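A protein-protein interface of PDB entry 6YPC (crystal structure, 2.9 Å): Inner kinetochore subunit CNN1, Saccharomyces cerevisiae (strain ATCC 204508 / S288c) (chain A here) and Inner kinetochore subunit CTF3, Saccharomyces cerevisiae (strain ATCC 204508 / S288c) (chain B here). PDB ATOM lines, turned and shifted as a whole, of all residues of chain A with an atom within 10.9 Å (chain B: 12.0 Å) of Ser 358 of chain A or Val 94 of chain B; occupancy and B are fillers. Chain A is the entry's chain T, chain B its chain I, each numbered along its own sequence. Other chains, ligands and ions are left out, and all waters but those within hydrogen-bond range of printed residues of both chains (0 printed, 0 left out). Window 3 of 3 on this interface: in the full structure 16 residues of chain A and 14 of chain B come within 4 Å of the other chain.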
ATOM      1  N   GLN A 322       9.441 -10.949   6.652  1.00  0.00           N
ATOM      2  CA  GLN A 322       9.685 -10.746   8.080  1.00  0.00           C
ATOM      3  C   GLN A 322      10.730 -11.715   8.627  1.00  0.00           C
ATOM      4  O   GLN A 322      11.639 -11.309   9.364  1.00  0.00           O
ATOM      5  CB  GLN A 322       8.366 -10.900   8.849  1.00  0.00           C
ATOM      6  CG  GLN A 322       7.179 -10.122   8.263  1.00  0.00           C
ATOM      7  CD  GLN A 322       7.099  -8.672   8.737  1.00  0.00           C
ATOM      8  OE1 GLN A 322       7.918  -8.213   9.541  1.00  0.00           O
ATOM      9  NE2 GLN A 322       6.092  -7.949   8.246  1.00  0.00           N
ATOM     10  N   VAL A 337      18.615  -7.323  14.434  1.00  0.00           N
ATOM     11  CA  VAL A 337      18.721  -6.702  13.119  1.00  0.00           C
ATOM     12  C   VAL A 337      19.815  -5.625  13.100  1.00  0.00           C
ATOM     13  O   VAL A 337      20.358  -5.295  12.039  1.00  0.00           O
ATOM     14  CB  VAL A 337      17.357  -6.126  12.713  1.00  0.00           C
ATOM     15  CG1 VAL A 337      16.877  -5.159  13.749  1.00  0.00           C
ATOM     16  CG2 VAL A 337      17.397  -5.469  11.351  1.00  0.00           C
ATOM     17  N   MET A 340      22.592  -7.134  11.539  1.00  0.00           N
ATOM     18  CA  MET A 340      22.474  -7.270  10.094  1.00  0.00           C
ATOM     19  C   MET A 340      22.926  -6.001   9.395  1.00  0.00           C
ATOM     20  O   MET A 340      23.475  -6.052   8.290  1.00  0.00           O
ATOM     21  CB  MET A 340      21.037  -7.607   9.703  1.00  0.00           C
ATOM     22  CG  MET A 340      20.830  -7.757   8.205  1.00  0.00           C
ATOM     23  SD  MET A 340      21.744  -9.147   7.492  1.00  0.00           S
ATOM     24  CE  MET A 340      20.620 -10.465   7.906  1.00  0.00           C
ATOM     25  N   PHE A 341      22.700  -4.854  10.021  1.00  0.00           N
ATOM     26  CA  PHE A 341      23.123  -3.606   9.407  1.00  0.00           C
ATOM     27  C   PHE A 341      24.639  -3.467   9.453  1.00  0.00           C
ATOM     28  O   PHE A 341      25.275  -3.119   8.450  1.00  0.00           O
ATOM     29  CB  PHE A 341      22.447  -2.433  10.092  1.00  0.00           C
ATOM     30  CG  PHE A 341      22.837  -1.120   9.519  1.00  0.00           C
ATOM     31  CD1 PHE A 341      22.251  -0.658   8.344  1.00  0.00           C
ATOM     32  CD2 PHE A 341      23.810  -0.352  10.132  1.00  0.00           C
ATOM     33  CE1 PHE A 341      22.607   0.566   7.805  1.00  0.00           C
ATOM     34  CE2 PHE A 341      24.169   0.864   9.607  1.00  0.00           C
ATOM     35  CZ  PHE A 341      23.567   1.326   8.438  1.00  0.00           C
ATOM     36  N   ALA A 344      25.517  -5.208   6.533  1.00  0.00           N
ATOM     37  CA  ALA A 344      25.302  -4.392   5.352  1.00  0.00           C
ATOM     38  C   ALA A 344      26.445  -3.416   5.175  1.00  0.00           C
ATOM     39  O   ALA A 344      27.005  -3.284   4.083  1.00  0.00           O
ATOM     40  CB  ALA A 344      23.974  -3.647   5.473  1.00  0.00           C
ATOM     41  N   LEU A 348      28.031  -4.190   1.659  1.00  0.00           N
ATOM     42  CA  LEU A 348      27.383  -3.450   0.589  1.00  0.00           C
ATOM     43  C   LEU A 348      28.088  -2.128   0.330  1.00  0.00           C
ATOM     44  O   LEU A 348      28.671  -1.537   1.244  1.00  0.00           O
ATOM     45  CB  LEU A 348      25.927  -3.173   0.949  1.00  0.00           C
ATOM     46  CG  LEU A 348      25.157  -4.486   0.992  1.00  0.00           C
ATOM     47  CD1 LEU A 348      23.672  -4.256   1.279  1.00  0.00           C
ATOM     48  CD2 LEU A 348      25.379  -5.194  -0.336  1.00  0.00           C
ATOM     49  N   LEU A 350      28.122   1.987  -0.513  1.00  0.00           N
ATOM     50  CA  LEU A 350      27.485   3.039   0.262  1.00  0.00           C
ATOM     51  C   LEU A 350      25.982   3.101   0.039  1.00  0.00           C
ATOM     52  O   LEU A 350      25.195   2.948   0.976  1.00  0.00           O
ATOM     53  CB  LEU A 350      28.118   4.390  -0.083  1.00  0.00           C
ATOM     54  CG  LEU A 350      27.914   5.434   1.009  1.00  0.00           C
ATOM     55  CD1 LEU A 350      28.541   4.881   2.263  1.00  0.00           C
ATOM     56  CD2 LEU A 350      28.549   6.763   0.624  1.00  0.00           C
ATOM     57  N   GLU A 351      25.576   3.312  -1.211  1.00  0.00           N
ATOM     58  CA  GLU A 351      24.198   3.685  -1.504  1.00  0.00           C
ATOM     59  C   GLU A 351      23.230   2.552  -1.205  1.00  0.00           C
ATOM     60  O   GLU A 351      22.086   2.804  -0.798  1.00  0.00           O
ATOM     61  CB  GLU A 351      24.088   4.122  -2.960  1.00  0.00           C
ATOM     62  CG  GLU A 351      24.394   3.012  -3.965  1.00  0.00           C
ATOM     63  CD  GLU A 351      25.893   2.746  -4.163  1.00  0.00           C
ATOM     64  OE1 GLU A 351      26.300   2.502  -5.316  1.00  0.00           O
ATOM     65  OE2 GLU A 351      26.668   2.761  -3.180  1.00  0.00           O
ATOM     66  N   LEU A 352      23.660   1.304  -1.378  1.00  0.00           N
ATOM     67  CA  LEU A 352      22.812   0.218  -0.923  1.00  0.00           C
ATOM     68  C   LEU A 352      22.691   0.212   0.586  1.00  0.00           C
ATOM     69  O   LEU A 352      21.680  -0.252   1.114  1.00  0.00           O
ATOM     70  CB  LEU A 352      23.352  -1.107  -1.427  1.00  0.00           C
ATOM     71  CG  LEU A 352      23.044  -1.193  -2.918  1.00  0.00           C
ATOM     72  CD1 LEU A 352      23.580  -2.491  -3.526  1.00  0.00           C
ATOM     73  CD2 LEU A 352      21.536  -1.047  -3.140  1.00  0.00           C
ATOM     74  N   GLN A 353      23.696   0.719   1.298  1.00  0.00           N
ATOM     75  CA  GLN A 353      23.593   0.767   2.750  1.00  0.00           C
ATOM     76  C   GLN A 353      22.443   1.660   3.166  1.00  0.00           C
ATOM     77  O   GLN A 353      21.593   1.256   3.969  1.00  0.00           O
ATOM     78  CB  GLN A 353      24.898   1.244   3.372  1.00  0.00           C
ATOM     79  CG  GLN A 353      26.022   0.285   3.143  1.00  0.00           C
ATOM     80  CD  GLN A 353      27.328   0.789   3.686  1.00  0.00           C
ATOM     81  OE1 GLN A 353      27.363   1.738   4.466  1.00  0.00           O
ATOM     82  NE2 GLN A 353      28.421   0.150   3.282  1.00  0.00           N
ATOM     83  N   SER A 354      22.376   2.868   2.604  1.00  0.00           N
ATOM     84  CA  SER A 354      21.243   3.733   2.900  1.00  0.00           C
ATOM     85  C   SER A 354      19.921   3.054   2.543  1.00  0.00           C
ATOM     86  O   SER A 354      18.941   3.197   3.276  1.00  0.00           O
ATOM     87  CB  SER A 354      21.390   5.077   2.175  1.00  0.00           C
ATOM     88  OG  SER A 354      22.694   5.640   2.345  1.00  0.00           O
ATOM     89  N   ARG A 355      19.875   2.273   1.459  1.00  0.00           N
ATOM     90  CA  ARG A 355      18.643   1.553   1.144  1.00  0.00           C
ATOM     91  C   ARG A 355      18.280   0.579   2.254  1.00  0.00           C
ATOM     92  O   ARG A 355      17.309   0.789   2.990  1.00  0.00           O
ATOM     93  CB  ARG A 355      18.771   0.805  -0.181  1.00  0.00           C
ATOM     94  CG  ARG A 355      17.459   0.177  -0.634  1.00  0.00           C
ATOM     95  CD  ARG A 355      17.644  -0.688  -1.875  1.00  0.00           C
ATOM     96  NE  ARG A 355      16.373  -0.929  -2.559  1.00  0.00           N
ATOM     97  CZ  ARG A 355      15.999  -0.320  -3.683  1.00  0.00           C
ATOM     98  NH1 ARG A 355      16.803   0.563  -4.260  1.00  0.00           N
ATOM     99  NH2 ARG A 355      14.820  -0.590  -4.231  1.00  0.00           N
ATOM    100  N   ILE A 356      19.065  -0.498   2.387  1.00  0.00           N
ATOM    101  CA  ILE A 356      18.850  -1.527   3.399  1.00  0.00           C
ATOM    102  C   ILE A 356      18.488  -0.933   4.749  1.00  0.00           C
ATOM    103  O   ILE A 356      17.669  -1.495   5.483  1.00  0.00           O
ATOM    104  CB  ILE A 356      20.104  -2.408   3.501  1.00  0.00           C
ATOM    105  CG1 ILE A 356      20.226  -3.275   2.265  1.00  0.00           C
ATOM    106  CG2 ILE A 356      20.030  -3.307   4.705  1.00  0.00           C
ATOM    107  CD1 ILE A 356      19.403  -4.532   2.335  1.00  0.00           C
ATOM    108  N   GLU A 357      19.081   0.209   5.105  1.00  0.00           N
ATOM    109  CA  GLU A 357      18.759   0.822   6.388  1.00  0.00           C
ATOM    110  C   GLU A 357      17.252   1.024   6.524  1.00  0.00           C
ATOM    111  O   GLU A 357      16.651   0.616   7.528  1.00  0.00           O
ATOM    112  CB  GLU A 357      19.508   2.148   6.560  1.00  0.00           C
ATOM    113  CG  GLU A 357      19.687   2.537   8.036  1.00  0.00           C
ATOM    114  CD  GLU A 357      20.072   4.009   8.275  1.00  0.00           C
ATOM    115  OE1 GLU A 357      20.668   4.643   7.366  1.00  0.00           O
ATOM    116  OE2 GLU A 357      19.742   4.538   9.377  1.00  0.00           O
ATOM    117  N   SER A 358      16.615   1.596   5.493  1.00  0.00           N
ATOM    118  CA  SER A 358      15.161   1.794   5.517  1.00  0.00           C
ATOM    119  C   SER A 358      14.380   0.473   5.451  1.00  0.00           C
ATOM    120  O   SER A 358      13.282   0.367   6.020  1.00  0.00           O
ATOM    121  CB  SER A 358      14.726   2.686   4.363  1.00  0.00           C
ATOM    122  OG  SER A 358      15.671   3.713   4.099  1.00  0.00           O
ATOM    123  N   TYR A 359      14.917  -0.544   4.768  1.00  0.00           N
ATOM    124  CA  TYR A 359      14.267  -1.848   4.770  1.00  0.00           C
ATOM    125  C   TYR A 359      14.183  -2.453   6.167  1.00  0.00           C
ATOM    126  O   TYR A 359      13.378  -3.363   6.385  1.00  0.00           O
ATOM    127  CB  TYR A 359      14.999  -2.803   3.832  1.00  0.00           C
ATOM    128  CG  TYR A 359      14.302  -4.136   3.734  1.00  0.00           C
ATOM    129  CD1 TYR A 359      14.927  -5.309   4.135  1.00  0.00           C
ATOM    130  CD2 TYR A 359      12.995  -4.216   3.281  1.00  0.00           C
ATOM    131  CE1 TYR A 359      14.277  -6.524   4.066  1.00  0.00           C
ATOM    132  CE2 TYR A 359      12.344  -5.421   3.210  1.00  0.00           C
ATOM    133  CZ  TYR A 359      12.980  -6.572   3.599  1.00  0.00           C
ATOM    134  OH  TYR A 359      12.297  -7.770   3.516  1.00  0.00           O
ATOM    135  N   LEU A 360      14.971  -1.966   7.120  1.00  0.00           N
ATOM    136  CA  LEU A 360      14.963  -2.535   8.468  1.00  0.00           C
ATOM    137  C   LEU A 360      14.395  -1.573   9.528  1.00  0.00           C
ATOM    138  O   LEU A 360      15.006  -0.554   9.892  1.00  0.00           O
ATOM    139  CB  LEU A 360      16.378  -2.971   8.838  1.00  0.00           C
ATOM    140  CG  LEU A 360      17.117  -3.667   7.692  1.00  0.00           C
ATOM    141  CD1 LEU A 360      18.519  -4.079   8.105  1.00  0.00           C
ATOM    142  CD2 LEU A 360      16.336  -4.869   7.229  1.00  0.00           C
ATOM    143  N   GLY B  90      24.006  11.850  -4.794  1.00  0.00           N
ATOM    144  CA  GLY B  90      23.912  10.971  -3.656  1.00  0.00           C
ATOM    145  C   GLY B  90      22.771   9.983  -3.803  1.00  0.00           C
ATOM    146  O   GLY B  90      22.293   9.708  -4.909  1.00  0.00           O
ATOM    147  N   THR B  91      22.350   9.442  -2.659  1.00  0.00           N
ATOM    148  CA  THR B  91      21.350   8.409  -2.486  1.00  0.00           C
ATOM    149  C   THR B  91      20.270   8.903  -1.522  1.00  0.00           C
ATOM    150  O   THR B  91      20.545   9.739  -0.647  1.00  0.00           O
ATOM    151  CB  THR B  91      21.997   7.129  -1.934  1.00  0.00           C
ATOM    152  OG1 THR B  91      21.036   6.073  -1.877  1.00  0.00           O
ATOM    153  CG2 THR B  91      22.522   7.366  -0.524  1.00  0.00           C
ATOM    154  N   PRO B  92      19.030   8.436  -1.670  1.00  0.00           N
ATOM    155  CA  PRO B  92      17.988   8.794  -0.697  1.00  0.00           C
ATOM    156  C   PRO B  92      18.242   8.112   0.638  1.00  0.00           C
ATOM    157  O   PRO B  92      18.405   6.894   0.704  1.00  0.00           O
ATOM    158  CB  PRO B  92      16.703   8.277  -1.347  1.00  0.00           C
ATOM    159  CG  PRO B  92      17.074   7.965  -2.746  1.00  0.00           C
ATOM    160  CD  PRO B  92      18.498   7.586  -2.739  1.00  0.00           C
ATOM    161  N   THR B  93      18.257   8.896   1.707  1.00  0.00           N
ATOM    162  CA  THR B  93      18.579   8.357   3.013  1.00  0.00           C
ATOM    163  C   THR B  93      17.427   8.581   3.990  1.00  0.00           C
ATOM    164  O   THR B  93      16.512   9.363   3.732  1.00  0.00           O
ATOM    165  CB  THR B  93      19.875   8.979   3.546  1.00  0.00           C
ATOM    166  OG1 THR B  93      20.214   8.340   4.783  1.00  0.00           O
ATOM    167  CG2 THR B  93      19.697  10.443   3.803  1.00  0.00           C
ATOM    168  N   VAL B  94      17.493   7.895   5.131  1.00  0.00           N
ATOM    169  CA  VAL B  94      16.417   7.912   6.121  1.00  0.00           C
ATOM    170  C   VAL B  94      16.097   9.325   6.603  1.00  0.00           C
ATOM    171  O   VAL B  94      15.044   9.555   7.208  1.00  0.00           O
ATOM    172  CB  VAL B  94      16.739   7.003   7.324  1.00  0.00           C
ATOM    173  CG1 VAL B  94      16.800   5.549   6.892  1.00  0.00           C
ATOM    174  CG2 VAL B  94      18.032   7.416   7.982  1.00  0.00           C
ATOM    175  N   PHE B  95      16.980  10.280   6.366  1.00  0.00           N
ATOM    176  CA  PHE B  95      16.632  11.659   6.677  1.00  0.00           C
ATOM    177  C   PHE B  95      16.126  12.406   5.456  1.00  0.00           C
ATOM    178  O   PHE B  95      15.825  13.600   5.552  1.00  0.00           O
ATOM    179  CB  PHE B  95      17.827  12.425   7.273  1.00  0.00           C
ATOM    180  CG  PHE B  95      18.481  11.754   8.454  1.00  0.00           C
ATOM    181  CD1 PHE B  95      19.275  10.630   8.290  1.00  0.00           C
ATOM    182  CD2 PHE B  95      18.344  12.279   9.708  1.00  0.00           C
ATOM    183  CE1 PHE B  95      19.886  10.022   9.354  1.00  0.00           C
ATOM    184  CE2 PHE B  95      18.951  11.665  10.786  1.00  0.00           C
ATOM    185  CZ  PHE B  95      19.721  10.529  10.603  1.00  0.00           C
ATOM    186  N   SER B  96      16.031  11.727   4.317  1.00  0.00           N
ATOM    187  CA  SER B  96      15.873  12.389   3.033  1.00  0.00           C
ATOM    188  C   SER B  96      15.023  11.520   2.115  1.00  0.00           C
ATOM    189  O   SER B  96      15.302  11.362   0.926  1.00  0.00           O
ATOM    190  CB  SER B  96      17.246  12.710   2.439  1.00  0.00           C
ATOM    191  OG  SER B  96      17.803  11.645   1.672  1.00  0.00           O
ATOM    192  N   ARG B  97      13.941  10.969   2.665  1.00  0.00           N
ATOM    193  CA  ARG B  97      13.092  10.084   1.874  1.00  0.00           C
ATOM    194  C   ARG B  97      12.064  10.861   1.056  1.00  0.00           C
ATOM    195  O   ARG B  97      11.665  10.401  -0.019  1.00  0.00           O
ATOM    196  CB  ARG B  97      12.418   9.040   2.775  1.00  0.00           C
ATOM    197  CG  ARG B  97      11.241   9.538   3.604  1.00  0.00           C
ATOM    198  CD  ARG B  97       9.888   9.318   2.886  1.00  0.00           C
ATOM    199  NE  ARG B  97       8.740   9.674   3.725  1.00  0.00           N
ATOM    200  CZ  ARG B  97       8.045  10.808   3.632  1.00  0.00           C
ATOM    201  NH1 ARG B  97       8.371  11.734   2.733  1.00  0.00           N
ATOM    202  NH2 ARG B  97       7.019  11.022   4.451  1.00  0.00           N
ATOM    203  N   TYR B  98      11.640  12.029   1.539  1.00  0.00           N
ATOM    204  CA  TYR B  98      10.815  13.009   0.838  1.00  0.00           C
ATOM    205  C   TYR B  98      11.548  13.718  -0.304  1.00  0.00           C
ATOM    206  O   TYR B  98      10.969  14.616  -0.936  1.00  0.00           O
ATOM    207  CB  TYR B  98      10.354  14.066   1.839  1.00  0.00           C
ATOM    208  CG  TYR B  98      11.541  14.847   2.429  1.00  0.00           C
ATOM    209  CD1 TYR B  98      12.427  14.231   3.346  1.00  0.00           C
ATOM    210  CD2 TYR B  98      11.794  16.190   2.061  1.00  0.00           C
ATOM    211  CE1 TYR B  98      13.518  14.915   3.879  1.00  0.00           C
ATOM    212  CE2 TYR B  98      12.892  16.889   2.602  1.00  0.00           C
ATOM    213  CZ  TYR B  98      13.741  16.235   3.515  1.00  0.00           C
ATOM    214  OH  TYR B  98      14.825  16.872   4.069  1.00  0.00           O
ATOM    215  N   ARG B  99      12.806  13.383  -0.559  1.00  0.00           N
ATOM    216  CA  ARG B  99      13.637  14.161  -1.454  1.00  0.00           C
ATOM    217  C   ARG B  99      13.384  13.717  -2.893  1.00  0.00           C
ATOM    218  O   ARG B  99      13.104  12.542  -3.155  1.00  0.00           O
ATOM    219  CB  ARG B  99      15.108  13.997  -1.048  1.00  0.00           C
ATOM    220  CG  ARG B  99      16.148  14.757  -1.873  1.00  0.00           C
ATOM    221  CD  ARG B  99      17.566  14.402  -1.399  1.00  0.00           C
ATOM    222  NE  ARG B  99      18.600  15.137  -2.134  1.00  0.00           N
ATOM    223  CZ  ARG B  99      19.902  14.844  -2.111  1.00  0.00           C
ATOM    224  NH1 ARG B  99      20.763  15.571  -2.821  1.00  0.00           N
ATOM    225  NH2 ARG B  99      20.349  13.813  -1.403  1.00  0.00           N
ATOM    226  N   ILE B 100      13.413  14.677  -3.815  1.00  0.00           N
ATOM    227  CA  ILE B 100      13.425  14.352  -5.235  1.00  0.00           C
ATOM    228  C   ILE B 100      14.805  13.780  -5.529  1.00  0.00           C
ATOM    229  O   ILE B 100      15.798  14.508  -5.456  1.00  0.00           O
ATOM    230  CB  ILE B 100      13.150  15.584  -6.107  1.00  0.00           C
ATOM    231  CG1 ILE B 100      12.159  16.538  -5.433  1.00  0.00           C
ATOM    232  CG2 ILE B 100      12.687  15.152  -7.496  1.00  0.00           C
ATOM    233  CD1 ILE B 100      12.070  17.908  -6.102  1.00  0.00           C
ATOM    234  N   GLN B 101      14.896  12.489  -5.835  1.00  0.00           N
ATOM    235  CA  GLN B 101      16.234  12.004  -6.140  1.00  0.00           C
ATOM    236  C   GLN B 101      16.393  11.717  -7.618  1.00  0.00           C
ATOM    237  O   GLN B 101      15.439  11.381  -8.323  1.00  0.00           O
ATOM    238  CB  GLN B 101      16.644  10.786  -5.313  1.00  0.00           C
ATOM    239  CG  GLN B 101      17.708  11.200  -4.239  1.00  0.00           C
ATOM    240  CD  GLN B 101      19.065  11.638  -4.858  1.00  0.00           C
ATOM    241  OE1 GLN B 101      19.755  10.830  -5.484  1.00  0.00           O
ATOM    242  NE2 GLN B 101      19.421  12.927  -4.706  1.00  0.00           N
ATOM    243  N   PHE B 142      30.271   6.758  -3.421  1.00  0.00           N
ATOM    244  CA  PHE B 142      29.097   6.219  -4.104  1.00  0.00           C
ATOM    245  C   PHE B 142      29.538   5.374  -5.285  1.00  0.00           C
ATOM    246  O   PHE B 142      30.150   5.887  -6.228  1.00  0.00           O
ATOM    247  CB  PHE B 142      28.178   7.340  -4.562  1.00  0.00           C
ATOM    248  CG  PHE B 142      27.410   7.950  -3.445  1.00  0.00           C
ATOM    249  CD1 PHE B 142      26.388   7.248  -2.838  1.00  0.00           C
ATOM    250  CD2 PHE B 142      27.725   9.205  -2.966  1.00  0.00           C
ATOM    251  CE1 PHE B 142      25.686   7.797  -1.786  1.00  0.00           C
ATOM    252  CE2 PHE B 142      27.014   9.754  -1.912  1.00  0.00           C
ATOM    253  CZ  PHE B 142      25.993   9.047  -1.327  1.00  0.00           C
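CD2 of Leu 350 of chain A touches CE1 of Phe 142 of chain B, 3.9 Å away. OG1 of Thr 91 of chain B touches O of Glu 351 of chain A, 3.6 Å away. Phe 142 of chain B touches Glu 351 of chain A (CD1 to CB, 3.9 Å). Thr 91 of chain B touches Ser 354 of chain A (CG2 to OG, 3.4 Å). Ser 354 of chain A touches Pro 92 of chain B (CB to O, 3.8 Å). Glu 357 of chain A touches Val 94 of chain B. Val 94 of chain B touches Ser 358 of chain A (CG1 to OG, 3.5 Å).
Phe 341 of chain A touches none of the printed residues of chain B. Of the printed residues of chain B, Glu 351 of chain A touches Thr 91 and Phe 142. No residue of chain B comes within 4 Å of Ile 356 of chain A. Glu 357 of chain A touches just one residue of chain B: Val 94. Of chain B, only Val 94 (3.5 Å) comes within 4 Å of Ser 358 of chain A. Leu 360 of chain A touches none of the printed residues of chain B. No residue of chain A comes within 4 Å of Thr 93 of chain B. Of chain A, only Glu 357 and Ser 358 come within 4 Å of Val 94 of chain B. No residue of chain A comes within 4 Å of Ser 96 of chain B. Arg 99 of chain B touches none of the printed residues of chain A. Of the printed residues of chain A, Phe 142 of chain B touches Leu 350 (3.9 Å) and Glu 351 (3.9 Å). The nearest residue of chain B that does not touch Ser 358 of chain A is Thr 93 of chain B (5.2 Å). The nearest printed residue of chain B that does not touch Glu 351 of chain A is Pro 92 of chain B (5.7 Å).
Of the 13 printed residues of chain B, 4 touch a printed residue of chain A. Printed residues of chain B that touch a printed residue of chain A: Thr 91, Pro 92, Val 94 and Phe 142. Hydrophobic or aromatic side chains of chain B within 4 Å of the printed part of chain A: Val 94 and Phe 142. Along chain B the printed residues that touch a printed residue of chain A span positions 91 to 142. Of the 17 printed residues of chain A, 5 touch a printed residue of chain B. Hydrophobic or aromatic side chains of chain A within 4 Å of the printed part of chain B: Leu 350. Among the printed residues, no Asp or Glu carboxylate lies within 4 Å of a Lys or Arg side-chain nitrogen of the other chain.
The side-chain hydroxyl (OG) of Ser 358 of chain A is in hydrogen-bond range of the backbone carbonyl oxygen (O) of Ser 354 of chain A.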
